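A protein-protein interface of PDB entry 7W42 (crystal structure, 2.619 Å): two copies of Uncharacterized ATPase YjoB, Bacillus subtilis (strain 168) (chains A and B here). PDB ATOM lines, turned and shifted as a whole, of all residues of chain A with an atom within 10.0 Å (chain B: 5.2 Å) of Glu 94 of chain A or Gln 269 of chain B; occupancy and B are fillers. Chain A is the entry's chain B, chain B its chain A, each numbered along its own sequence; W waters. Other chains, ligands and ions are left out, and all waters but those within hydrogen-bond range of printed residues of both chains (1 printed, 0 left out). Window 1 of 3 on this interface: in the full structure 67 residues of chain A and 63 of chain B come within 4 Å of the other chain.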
ATOM      1  N   ALA A  89      35.538 -13.997  20.703  1.00  0.00           N
ATOM      2  CA  ALA A  89      34.342 -13.323  20.250  1.00  0.00           C
ATOM      3  C   ALA A  89      34.102 -13.517  18.763  1.00  0.00           C
ATOM      4  O   ALA A  89      32.994 -13.248  18.300  1.00  0.00           O
ATOM      5  CB  ALA A  89      34.450 -11.840  20.617  1.00  0.00           C
ATOM      6  N   TYR A  90      35.103 -14.008  18.029  1.00  0.00           N
ATOM      7  CA  TYR A  90      35.126 -14.070  16.570  1.00  0.00           C
ATOM      8  C   TYR A  90      33.975 -14.862  15.986  1.00  0.00           C
ATOM      9  O   TYR A  90      33.937 -16.090  16.113  1.00  0.00           O
ATOM     10  CB  TYR A  90      36.441 -14.685  16.091  1.00  0.00           C
ATOM     11  CG  TYR A  90      36.501 -14.938  14.607  1.00  0.00           C
ATOM     12  CD1 TYR A  90      36.848 -13.917  13.730  1.00  0.00           C
ATOM     13  CD2 TYR A  90      36.203 -16.187  14.076  1.00  0.00           C
ATOM     14  CE1 TYR A  90      36.924 -14.135  12.362  1.00  0.00           C
ATOM     15  CE2 TYR A  90      36.266 -16.419  12.705  1.00  0.00           C
ATOM     16  CZ  TYR A  90      36.636 -15.393  11.858  1.00  0.00           C
ATOM     17  OH  TYR A  90      36.707 -15.612  10.506  1.00  0.00           O
ATOM     18  N   ASP A  91      33.062 -14.157  15.323  1.00  0.00           N
ATOM     19  CA  ASP A  91      31.907 -14.746  14.664  1.00  0.00           C
ATOM     20  C   ASP A  91      31.942 -14.337  13.196  1.00  0.00           C
ATOM     21  O   ASP A  91      31.780 -13.154  12.871  1.00  0.00           O
ATOM     22  CB  ASP A  91      30.610 -14.297  15.344  1.00  0.00           C
ATOM     23  CG  ASP A  91      29.361 -15.008  14.797  1.00  0.00           C
ATOM     24  OD1 ASP A  91      29.423 -15.640  13.708  1.00  0.00           O
ATOM     25  OD2 ASP A  91      28.303 -14.917  15.472  1.00  0.00           O
ATOM     26  N   GLU A  92      32.153 -15.321  12.314  1.00  0.00           N
ATOM     27  CA  GLU A  92      32.333 -15.047  10.891  1.00  0.00           C
ATOM     28  C   GLU A  92      31.063 -14.518  10.238  1.00  0.00           C
ATOM     29  O   GLU A  92      31.140 -13.905   9.164  1.00  0.00           O
ATOM     30  CB  GLU A  92      32.802 -16.313  10.171  1.00  0.00           C
ATOM     31  CG  GLU A  92      31.830 -17.471  10.309  1.00  0.00           C
ATOM     32  CD  GLU A  92      32.394 -18.772   9.777  1.00  0.00           C
ATOM     33  OE1 GLU A  92      33.630 -18.849   9.573  1.00  0.00           O
ATOM     34  OE2 GLU A  92      31.604 -19.725   9.559  1.00  0.00           O
ATOM     35  N   ASP A  93      29.903 -14.752  10.855  1.00  0.00           N
ATOM     36  CA  ASP A  93      28.626 -14.262  10.360  1.00  0.00           C
ATOM     37  C   ASP A  93      28.291 -12.870  10.886  1.00  0.00           C
ATOM     38  O   ASP A  93      27.125 -12.460  10.842  1.00  0.00           O
ATOM     39  CB  ASP A  93      27.521 -15.255  10.719  1.00  0.00           C
ATOM     40  CG  ASP A  93      27.673 -16.573   9.981  1.00  0.00           C
ATOM     41  OD1 ASP A  93      28.072 -16.556   8.788  1.00  0.00           O
ATOM     42  OD2 ASP A  93      27.407 -17.623  10.599  1.00  0.00           O
ATOM     43  N   GLU A  94      29.296 -12.146  11.386  1.00  0.00           N
ATOM     44  CA  GLU A  94      29.167 -10.790  11.899  1.00  0.00           C
ATOM     45  C   GLU A  94      30.064  -9.866  11.075  1.00  0.00           C
ATOM     46  O   GLU A  94      31.184 -10.242  10.715  1.00  0.00           O
ATOM     47  CB  GLU A  94      29.544 -10.754  13.393  1.00  0.00           C
ATOM     48  CG  GLU A  94      30.079  -9.424  13.889  1.00  0.00           C
ATOM     49  CD  GLU A  94      28.965  -8.435  14.211  1.00  0.00           C
ATOM     50  OE1 GLU A  94      29.075  -7.245  13.808  1.00  0.00           O
ATOM     51  OE2 GLU A  94      27.975  -8.857  14.863  1.00  0.00           O
ATOM     52  N   LYS A  95      29.574  -8.663  10.759  1.00  0.00           N
ATOM     53  CA  LYS A  95      30.319  -7.787   9.853  1.00  0.00           C
ATOM     54  C   LYS A  95      31.608  -7.268  10.497  1.00  0.00           C
ATOM     55  O   LYS A  95      32.627  -7.114   9.814  1.00  0.00           O
ATOM     56  CB  LYS A  95      29.433  -6.621   9.401  1.00  0.00           C
ATOM     57  CG  LYS A  95      28.020  -7.039   8.978  1.00  0.00           C
ATOM     58  CD  LYS A  95      27.196  -5.842   8.528  1.00  0.00           C
ATOM     59  CE  LYS A  95      25.828  -6.289   8.030  1.00  0.00           C
ATOM     60  NZ  LYS A  95      25.131  -5.253   7.209  1.00  0.00           N
ATOM     61  N   GLU A  96      31.581  -6.984  11.810  1.00  0.00           N
ATOM     62  CA  GLU A  96      32.746  -6.547  12.565  1.00  0.00           C
ATOM     63  C   GLU A  96      33.411  -7.739  13.231  1.00  0.00           C
ATOM     64  O   GLU A  96      32.914  -8.206  14.262  1.00  0.00           O
ATOM     65  CB  GLU A  96      32.348  -5.500  13.622  1.00  0.00           C
ATOM     66  CG  GLU A  96      31.255  -4.506  13.201  1.00  0.00           C
ATOM     67  CD  GLU A  96      31.128  -3.301  14.160  1.00  0.00           C
ATOM     68  OE1 GLU A  96      31.633  -2.197  13.823  1.00  0.00           O
ATOM     69  OE2 GLU A  96      30.517  -3.459  15.250  1.00  0.00           O
ATOM     70  N   PRO A  97      34.519  -8.262  12.702  1.00  0.00           N
ATOM     71  CA  PRO A  97      35.168  -9.400  13.367  1.00  0.00           C
ATOM     72  C   PRO A  97      35.852  -8.940  14.639  1.00  0.00           C
ATOM     73  O   PRO A  97      36.663  -8.009  14.627  1.00  0.00           O
ATOM     74  CB  PRO A  97      36.179  -9.911  12.326  1.00  0.00           C
ATOM     75  CG  PRO A  97      35.858  -9.159  11.064  1.00  0.00           C
ATOM     76  CD  PRO A  97      35.239  -7.878  11.478  1.00  0.00           C
ATOM     77  N   ASP A  98      35.490  -9.582  15.742  1.00  0.00           N
ATOM     78  CA  ASP A  98      36.071  -9.331  17.054  1.00  0.00           C
ATOM     79  C   ASP A  98      36.969 -10.512  17.360  1.00  0.00           C
ATOM     80  O   ASP A  98      36.491 -11.643  17.416  1.00  0.00           O
ATOM     81  CB  ASP A  98      34.983  -9.195  18.116  1.00  0.00           C
ATOM     82  CG  ASP A  98      35.445  -8.437  19.325  1.00  0.00           C
ATOM     83  OD1 ASP A  98      36.674  -8.386  19.552  1.00  0.00           O
ATOM     84  OD2 ASP A  98      34.580  -7.897  20.050  1.00  0.00           O
ATOM     85  N   TYR A  99      38.253 -10.260  17.536  1.00  0.00           N
ATOM     86  CA  TYR A  99      39.205 -11.330  17.764  1.00  0.00           C
ATOM     87  C   TYR A  99      39.579 -11.502  19.237  1.00  0.00           C
ATOM     88  O   TYR A  99      40.485 -12.276  19.543  1.00  0.00           O
ATOM     89  CB  TYR A  99      40.457 -11.073  16.918  1.00  0.00           C
ATOM     90  CG  TYR A  99      40.188 -11.136  15.428  1.00  0.00           C
ATOM     91  CD1 TYR A  99      39.721 -12.309  14.843  1.00  0.00           C
ATOM     92  CD2 TYR A  99      40.389 -10.025  14.606  1.00  0.00           C
ATOM     93  CE1 TYR A  99      39.477 -12.385  13.483  1.00  0.00           C
ATOM     94  CE2 TYR A  99      40.132 -10.091  13.227  1.00  0.00           C
ATOM     95  CZ  TYR A  99      39.671 -11.285  12.678  1.00  0.00           C
ATOM     96  OH  TYR A  99      39.412 -11.403  11.324  1.00  0.00           O
ATOM     97  N   LYS A 162      27.497   3.519  19.797  1.00  0.00           N
ATOM     98  CA  LYS A 162      27.180   2.587  18.732  1.00  0.00           C
ATOM     99  C   LYS A 162      26.212   3.311  17.807  1.00  0.00           C
ATOM    100  O   LYS A 162      25.572   4.277  18.209  1.00  0.00           O
ATOM    101  CB  LYS A 162      26.482   1.334  19.296  1.00  0.00           C
ATOM    102  CG  LYS A 162      27.355   0.349  20.083  1.00  0.00           C
ATOM    103  CD  LYS A 162      28.668   0.003  19.381  1.00  0.00           C
ATOM    104  CE  LYS A 162      28.501  -0.529  17.979  1.00  0.00           C
ATOM    105  NZ  LYS A 162      29.802  -0.529  17.246  1.00  0.00           N
ATOM    106  N   VAL A 163      26.047   2.841  16.580  1.00  0.00           N
ATOM    107  CA  VAL A 163      24.875   3.209  15.787  1.00  0.00           C
ATOM    108  C   VAL A 163      24.026   1.965  15.610  1.00  0.00           C
ATOM    109  O   VAL A 163      24.542   0.891  15.284  1.00  0.00           O
ATOM    110  CB  VAL A 163      25.225   3.844  14.428  1.00  0.00           C
ATOM    111  CG1 VAL A 163      25.786   5.241  14.640  1.00  0.00           C
ATOM    112  CG2 VAL A 163      26.158   2.975  13.599  1.00  0.00           C
ATOM    113  N   SER A 174      15.753  -6.669  11.768  1.00  0.00           N
ATOM    114  CA  SER A 174      17.023  -7.126  12.321  1.00  0.00           C
ATOM    115  C   SER A 174      17.766  -5.928  12.888  1.00  0.00           C
ATOM    116  O   SER A 174      17.864  -4.891  12.225  1.00  0.00           O
ATOM    117  CB  SER A 174      17.886  -7.810  11.256  1.00  0.00           C
ATOM    118  OG  SER A 174      17.352  -9.070  10.899  1.00  0.00           O
ATOM    119  N   ARG A 175      18.284  -6.070  14.106  1.00  0.00           N
ATOM    120  CA  ARG A 175      19.033  -5.016  14.781  1.00  0.00           C
ATOM    121  C   ARG A 175      20.521  -5.351  14.710  1.00  0.00           C
ATOM    122  O   ARG A 175      20.922  -6.496  14.957  1.00  0.00           O
ATOM    123  CB  ARG A 175      18.567  -4.865  16.234  1.00  0.00           C
ATOM    124  CG  ARG A 175      19.449  -4.005  17.181  1.00  0.00           C
ATOM    125  CD  ARG A 175      19.224  -4.391  18.680  1.00  0.00           C
ATOM    126  NE  ARG A 175      19.888  -3.483  19.619  1.00  0.00           N
ATOM    127  CZ  ARG A 175      19.286  -2.490  20.292  1.00  0.00           C
ATOM    128  NH1 ARG A 175      17.986  -2.255  20.148  1.00  0.00           N
ATOM    129  NH2 ARG A 175      19.989  -1.716  21.120  1.00  0.00           N
ATOM    130  N   GLU A 176      21.329  -4.366  14.326  1.00  0.00           N
ATOM    131  CA  GLU A 176      22.775  -4.513  14.295  1.00  0.00           C
ATOM    132  C   GLU A 176      23.378  -3.232  14.835  1.00  0.00           C
ATOM    133  O   GLU A 176      22.911  -2.140  14.500  1.00  0.00           O
ATOM    134  CB  GLU A 176      23.295  -4.800  12.874  1.00  0.00           C
ATOM    135  CG  GLU A 176      23.232  -6.293  12.513  1.00  0.00           C
ATOM    136  CD  GLU A 176      24.238  -6.710  11.442  1.00  0.00           C
ATOM    137  OE1 GLU A 176      23.818  -6.936  10.282  1.00  0.00           O
ATOM    138  OE2 GLU A 176      25.446  -6.825  11.762  1.00  0.00           O
ATOM    139  N   GLN A 177      24.397  -3.366  15.685  1.00  0.00           N
ATOM    140  CA  GLN A 177      25.052  -2.219  16.302  1.00  0.00           C
ATOM    141  C   GLN A 177      26.448  -2.115  15.716  1.00  0.00           C
ATOM    142  O   GLN A 177      27.316  -2.941  16.008  1.00  0.00           O
ATOM    143  CB  GLN A 177      25.052  -2.351  17.823  1.00  0.00           C
ATOM    144  CG  GLN A 177      23.621  -2.456  18.349  1.00  0.00           C
ATOM    145  CD  GLN A 177      23.500  -2.491  19.862  1.00  0.00           C
ATOM    146  OE1 GLN A 177      23.007  -3.473  20.435  1.00  0.00           O
ATOM    147  NE2 GLN A 177      23.923  -1.408  20.520  1.00  0.00           N
ATOM    148  N   GLU A 178      26.648  -1.126  14.861  1.00  0.00           N
ATOM    149  CA  GLU A 178      27.920  -0.895  14.199  1.00  0.00           C
ATOM    150  C   GLU A 178      28.523   0.412  14.693  1.00  0.00           C
ATOM    151  O   GLU A 178      27.847   1.252  15.290  1.00  0.00           O
ATOM    152  CB  GLU A 178      27.741  -0.828  12.677  1.00  0.00           C
ATOM    153  CG  GLU A 178      26.461  -1.489  12.126  1.00  0.00           C
ATOM    154  CD  GLU A 178      26.243  -1.228  10.619  1.00  0.00           C
ATOM    155  OE1 GLU A 178      26.518  -0.093  10.150  1.00  0.00           O
ATOM    156  OE2 GLU A 178      25.803  -2.168   9.908  1.00  0.00           O
ATOM    157  N   ALA A 179      29.815   0.587  14.455  1.00  0.00           N
ATOM    158  CA  ALA A 179      30.404   1.914  14.522  1.00  0.00           C
ATOM    159  C   ALA A 179      30.507   2.476  13.103  1.00  0.00           C
ATOM    160  O   ALA A 179      30.672   1.730  12.130  1.00  0.00           O
ATOM    161  CB  ALA A 179      31.767   1.887  15.228  1.00  0.00           C
ATOM    162  N   ILE B 264      20.683  -9.310  -1.310  1.00  0.00           N
ATOM    163  CA  ILE B 264      21.623  -8.201  -1.437  1.00  0.00           C
ATOM    164  C   ILE B 264      22.561  -8.153  -0.238  1.00  0.00           C
ATOM    165  O   ILE B 264      23.789  -8.129  -0.388  1.00  0.00           O
ATOM    166  CB  ILE B 264      20.868  -6.874  -1.597  1.00  0.00           C
ATOM    167  CG1 ILE B 264      19.984  -6.908  -2.859  1.00  0.00           C
ATOM    168  CG2 ILE B 264      21.871  -5.742  -1.641  1.00  0.00           C
ATOM    169  CD1 ILE B 264      19.050  -5.724  -3.017  1.00  0.00           C
ATOM    170  N   GLU B 265      22.000  -8.163   0.975  1.00  0.00           N
ATOM    171  CA  GLU B 265      22.848  -8.038   2.156  1.00  0.00           C
ATOM    172  C   GLU B 265      23.747  -9.255   2.331  1.00  0.00           C
ATOM    173  O   GLU B 265      24.905  -9.114   2.743  1.00  0.00           O
ATOM    174  CB  GLU B 265      22.007  -7.785   3.410  1.00  0.00           C
ATOM    175  CG  GLU B 265      22.154  -6.339   3.864  1.00  0.00           C
ATOM    176  CD  GLU B 265      21.568  -6.047   5.233  1.00  0.00           C
ATOM    177  OE1 GLU B 265      22.095  -5.123   5.903  1.00  0.00           O
ATOM    178  OE2 GLU B 265      20.580  -6.716   5.628  1.00  0.00           O
ATOM    179  N   GLU B 266      23.242 -10.452   2.005  1.00  0.00           N
ATOM    180  CA  GLU B 266      24.068 -11.654   2.073  1.00  0.00           C
ATOM    181  C   GLU B 266      25.269 -11.551   1.135  1.00  0.00           C
ATOM    182  O   GLU B 266      26.413 -11.812   1.541  1.00  0.00           O
ATOM    183  CB  GLU B 266      23.228 -12.881   1.735  1.00  0.00           C
ATOM    184  CG  GLU B 266      23.771 -14.172   2.336  1.00  0.00           C
ATOM    185  CD  GLU B 266      22.791 -15.330   2.205  1.00  0.00           C
ATOM    186  OE1 GLU B 266      21.907 -15.258   1.316  1.00  0.00           O
ATOM    187  OE2 GLU B 266      22.901 -16.303   2.991  1.00  0.00           O
ATOM    188  N   VAL B 267      25.023 -11.142  -0.120  1.00  0.00           N
ATOM    189  CA  VAL B 267      26.075 -11.065  -1.133  1.00  0.00           C
ATOM    190  C   VAL B 267      27.117 -10.018  -0.757  1.00  0.00           C
ATOM    191  O   VAL B 267      28.328 -10.263  -0.837  1.00  0.00           O
ATOM    192  CB  VAL B 267      25.452 -10.774  -2.509  1.00  0.00           C
ATOM    193  CG1 VAL B 267      26.516 -10.380  -3.519  1.00  0.00           C
ATOM    194  CG2 VAL B 267      24.652 -11.975  -2.987  1.00  0.00           C
ATOM    195  N   PHE B 268      26.668  -8.845  -0.323  1.00  0.00           N
ATOM    196  CA  PHE B 268      27.607  -7.786   0.010  1.00  0.00           C
ATOM    197  C   PHE B 268      28.423  -8.132   1.248  1.00  0.00           C
ATOM    198  O   PHE B 268      29.625  -7.848   1.296  1.00  0.00           O
ATOM    199  CB  PHE B 268      26.861  -6.468   0.174  1.00  0.00           C
ATOM    200  CG  PHE B 268      26.611  -5.773  -1.130  1.00  0.00           C
ATOM    201  CD1 PHE B 268      27.608  -5.013  -1.722  1.00  0.00           C
ATOM    202  CD2 PHE B 268      25.401  -5.900  -1.778  1.00  0.00           C
ATOM    203  CE1 PHE B 268      27.400  -4.388  -2.932  1.00  0.00           C
ATOM    204  CE2 PHE B 268      25.185  -5.270  -2.989  1.00  0.00           C
ATOM    205  CZ  PHE B 268      26.191  -4.515  -3.564  1.00  0.00           C
ATOM    206  N   GLN B 269      27.806  -8.777   2.243  1.00  0.00           N
ATOM    207  CA  GLN B 269      28.584  -9.223   3.396  1.00  0.00           C
ATOM    208  C   GLN B 269      29.569 -10.334   3.024  1.00  0.00           C
ATOM    209  O   GLN B 269      30.662 -10.412   3.602  1.00  0.00           O
ATOM    210  CB  GLN B 269      27.661  -9.684   4.526  1.00  0.00           C
ATOM    211  CG  GLN B 269      28.401  -9.950   5.858  1.00  0.00           C
ATOM    212  CD  GLN B 269      27.501 -10.537   6.950  1.00  0.00           C
ATOM    213  OE1 GLN B 269      26.266 -10.421   6.899  1.00  0.00           O
ATOM    214  NE2 GLN B 269      28.123 -11.170   7.949  1.00  0.00           N
ATOM    215  N   ALA B 270      29.211 -11.194   2.065  1.00  0.00           N
ATOM    216  CA  ALA B 270      30.129 -12.255   1.663  1.00  0.00           C
ATOM    217  C   ALA B 270      31.266 -11.708   0.801  1.00  0.00           C
ATOM    218  O   ALA B 270      32.424 -12.112   0.963  1.00  0.00           O
ATOM    219  CB  ALA B 270      29.365 -13.358   0.930  1.00  0.00           C
ATOM    220  N   ALA B 271      30.964 -10.785  -0.112  1.00  0.00           N
ATOM    221  CA  ALA B 271      32.035 -10.146  -0.864  1.00  0.00           C
ATOM    222  C   ALA B 271      32.951  -9.356   0.062  1.00  0.00           C
ATOM    223  O   ALA B 271      34.183  -9.427  -0.049  1.00  0.00           O
ATOM    224  CB  ALA B 271      31.453  -9.238  -1.942  1.00  0.00           C
ATOM    225  N   ARG B 272      32.357  -8.616   1.004  1.00  0.00           N
ATOM    226  CA  ARG B 272      33.127  -7.777   1.916  1.00  0.00           C
ATOM    227  C   ARG B 272      34.098  -8.573   2.769  1.00  0.00           C
ATOM    228  O   ARG B 272      35.072  -7.998   3.261  1.00  0.00           O
ATOM    229  CB  ARG B 272      32.201  -7.003   2.825  1.00  0.00           C
ATOM    230  CG  ARG B 272      32.629  -5.604   3.068  1.00  0.00           C
ATOM    231  CD  ARG B 272      31.390  -4.761   3.323  1.00  0.00           C
ATOM    232  NE  ARG B 272      31.028  -3.911   2.189  1.00  0.00           N
ATOM    233  CZ  ARG B 272      29.775  -3.620   1.848  1.00  0.00           C
ATOM    234  NH1 ARG B 272      28.757  -4.129   2.556  1.00  0.00           N
ATOM    235  NH2 ARG B 272      29.548  -2.819   0.803  1.00  0.00           N
ATOM    236  N   ARG B 273      33.858  -9.877   2.956  1.00  0.00           N
ATOM    237  CA  ARG B 273      34.832 -10.734   3.622  1.00  0.00           C
ATOM    238  C   ARG B 273      36.095 -10.938   2.795  1.00  0.00           C
ATOM    239  O   ARG B 273      37.160 -11.200   3.364  1.00  0.00           O
ATOM    240  CB  ARG B 273      34.182 -12.069   3.960  1.00  0.00           C
ATOM    241  CG  ARG B 273      33.015 -11.898   4.930  1.00  0.00           C
ATOM    242  CD  ARG B 273      32.567 -13.183   5.613  1.00  0.00           C
ATOM    243  NE  ARG B 273      31.834 -14.094   4.730  1.00  0.00           N
ATOM    244  CZ  ARG B 273      30.519 -14.294   4.775  1.00  0.00           C
ATOM    245  NH1 ARG B 273      29.761 -13.630   5.649  1.00  0.00           N
ATOM    246  NH2 ARG B 273      29.957 -15.158   3.932  1.00  0.00           N
HETATM  247  O   HOH W   1      30.717 -10.980   8.478  1.00  0.00           O
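The side-chain carboxylate of Glu 265 of chain B is in salt-bridge range of the side-chain amino group of Lys 95 of chain A. The side-chain amide nitrogen (NE2) of Gln 269 of chain B is in hydrogen-bond range of the backbone carbonyl oxygen (O) of Asp 93 of chain A (3.3 Å).
The side-chain carboxylate (OD1) of Asp 91 of chain A sits at hydrogen-bond distance from the backbone NH (N) of Asp 93 of chain A (3.0 Å). The backbone NH of Glu 96 of chain A sits at hydrogen-bond distance from the side-chain carboxylate of Glu 94 of chain A (3.2 Å). NZ of Lys 95 of chain A lies within salt-bridge range of OE1 of Glu 176 of chain A.
Among the printed residues, merely in contact across the chains: Glu 94 of chain A with Gln 269 of chain B (3.8 Å) and Glu 92 of chain A with Arg 273 of chain B (3.8 Å).
Glu 94 of chain A touches one residue of chain B. Of chain A, only Asp 93 and Glu 94 come within 4 Å of Gln 269 of chain B. No residue of chain A comes within 4 Å of Ala 271 of chain B. Of the printed residues of chain B, Lys 95 of chain A touches Glu 265. Of the printed residues of chain B, Glu 92 of chain A touches Arg 273 (3.8 Å). Of the printed residues of chain B, Asp 93 of chain A touches Gln 269 (3.3 Å). Of the printed residues of chain A, Glu 265 of chain B touches Lys 95 (3.3 Å). Of the printed residues of chain A, Arg 273 of chain B touches Glu 92.
Of the 19 printed residues of chain A, 4 touch a printed residue of chain B. Among the printed residues, 4 pairs touch across the chains. Among the printed residues, Asp or Glu carboxylates within 4 Å of a Lys or Arg side-chain nitrogen of the other chain: Lys 95 of chain A with Glu 265 of chain B (3.3 Å).
No position is printed for both chains. Of the 4 pairs that touch across the chains among the printed residues, none has its exchanged pair printed and touching as well.
Water W1 lies within hydrogen-bond range of the backbone carbonyl oxygen (O) of Glu 94 of chain A (2.4 Å), the side-chain amide nitrogen (NE2) of Gln 269 of chain B (2.7 Å), the backbone carbonyl oxygen (O) of Glu 92 of chain A (3.0 Å) and the backbone NH (N) of Lys 95 of chain A (3.4 Å).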
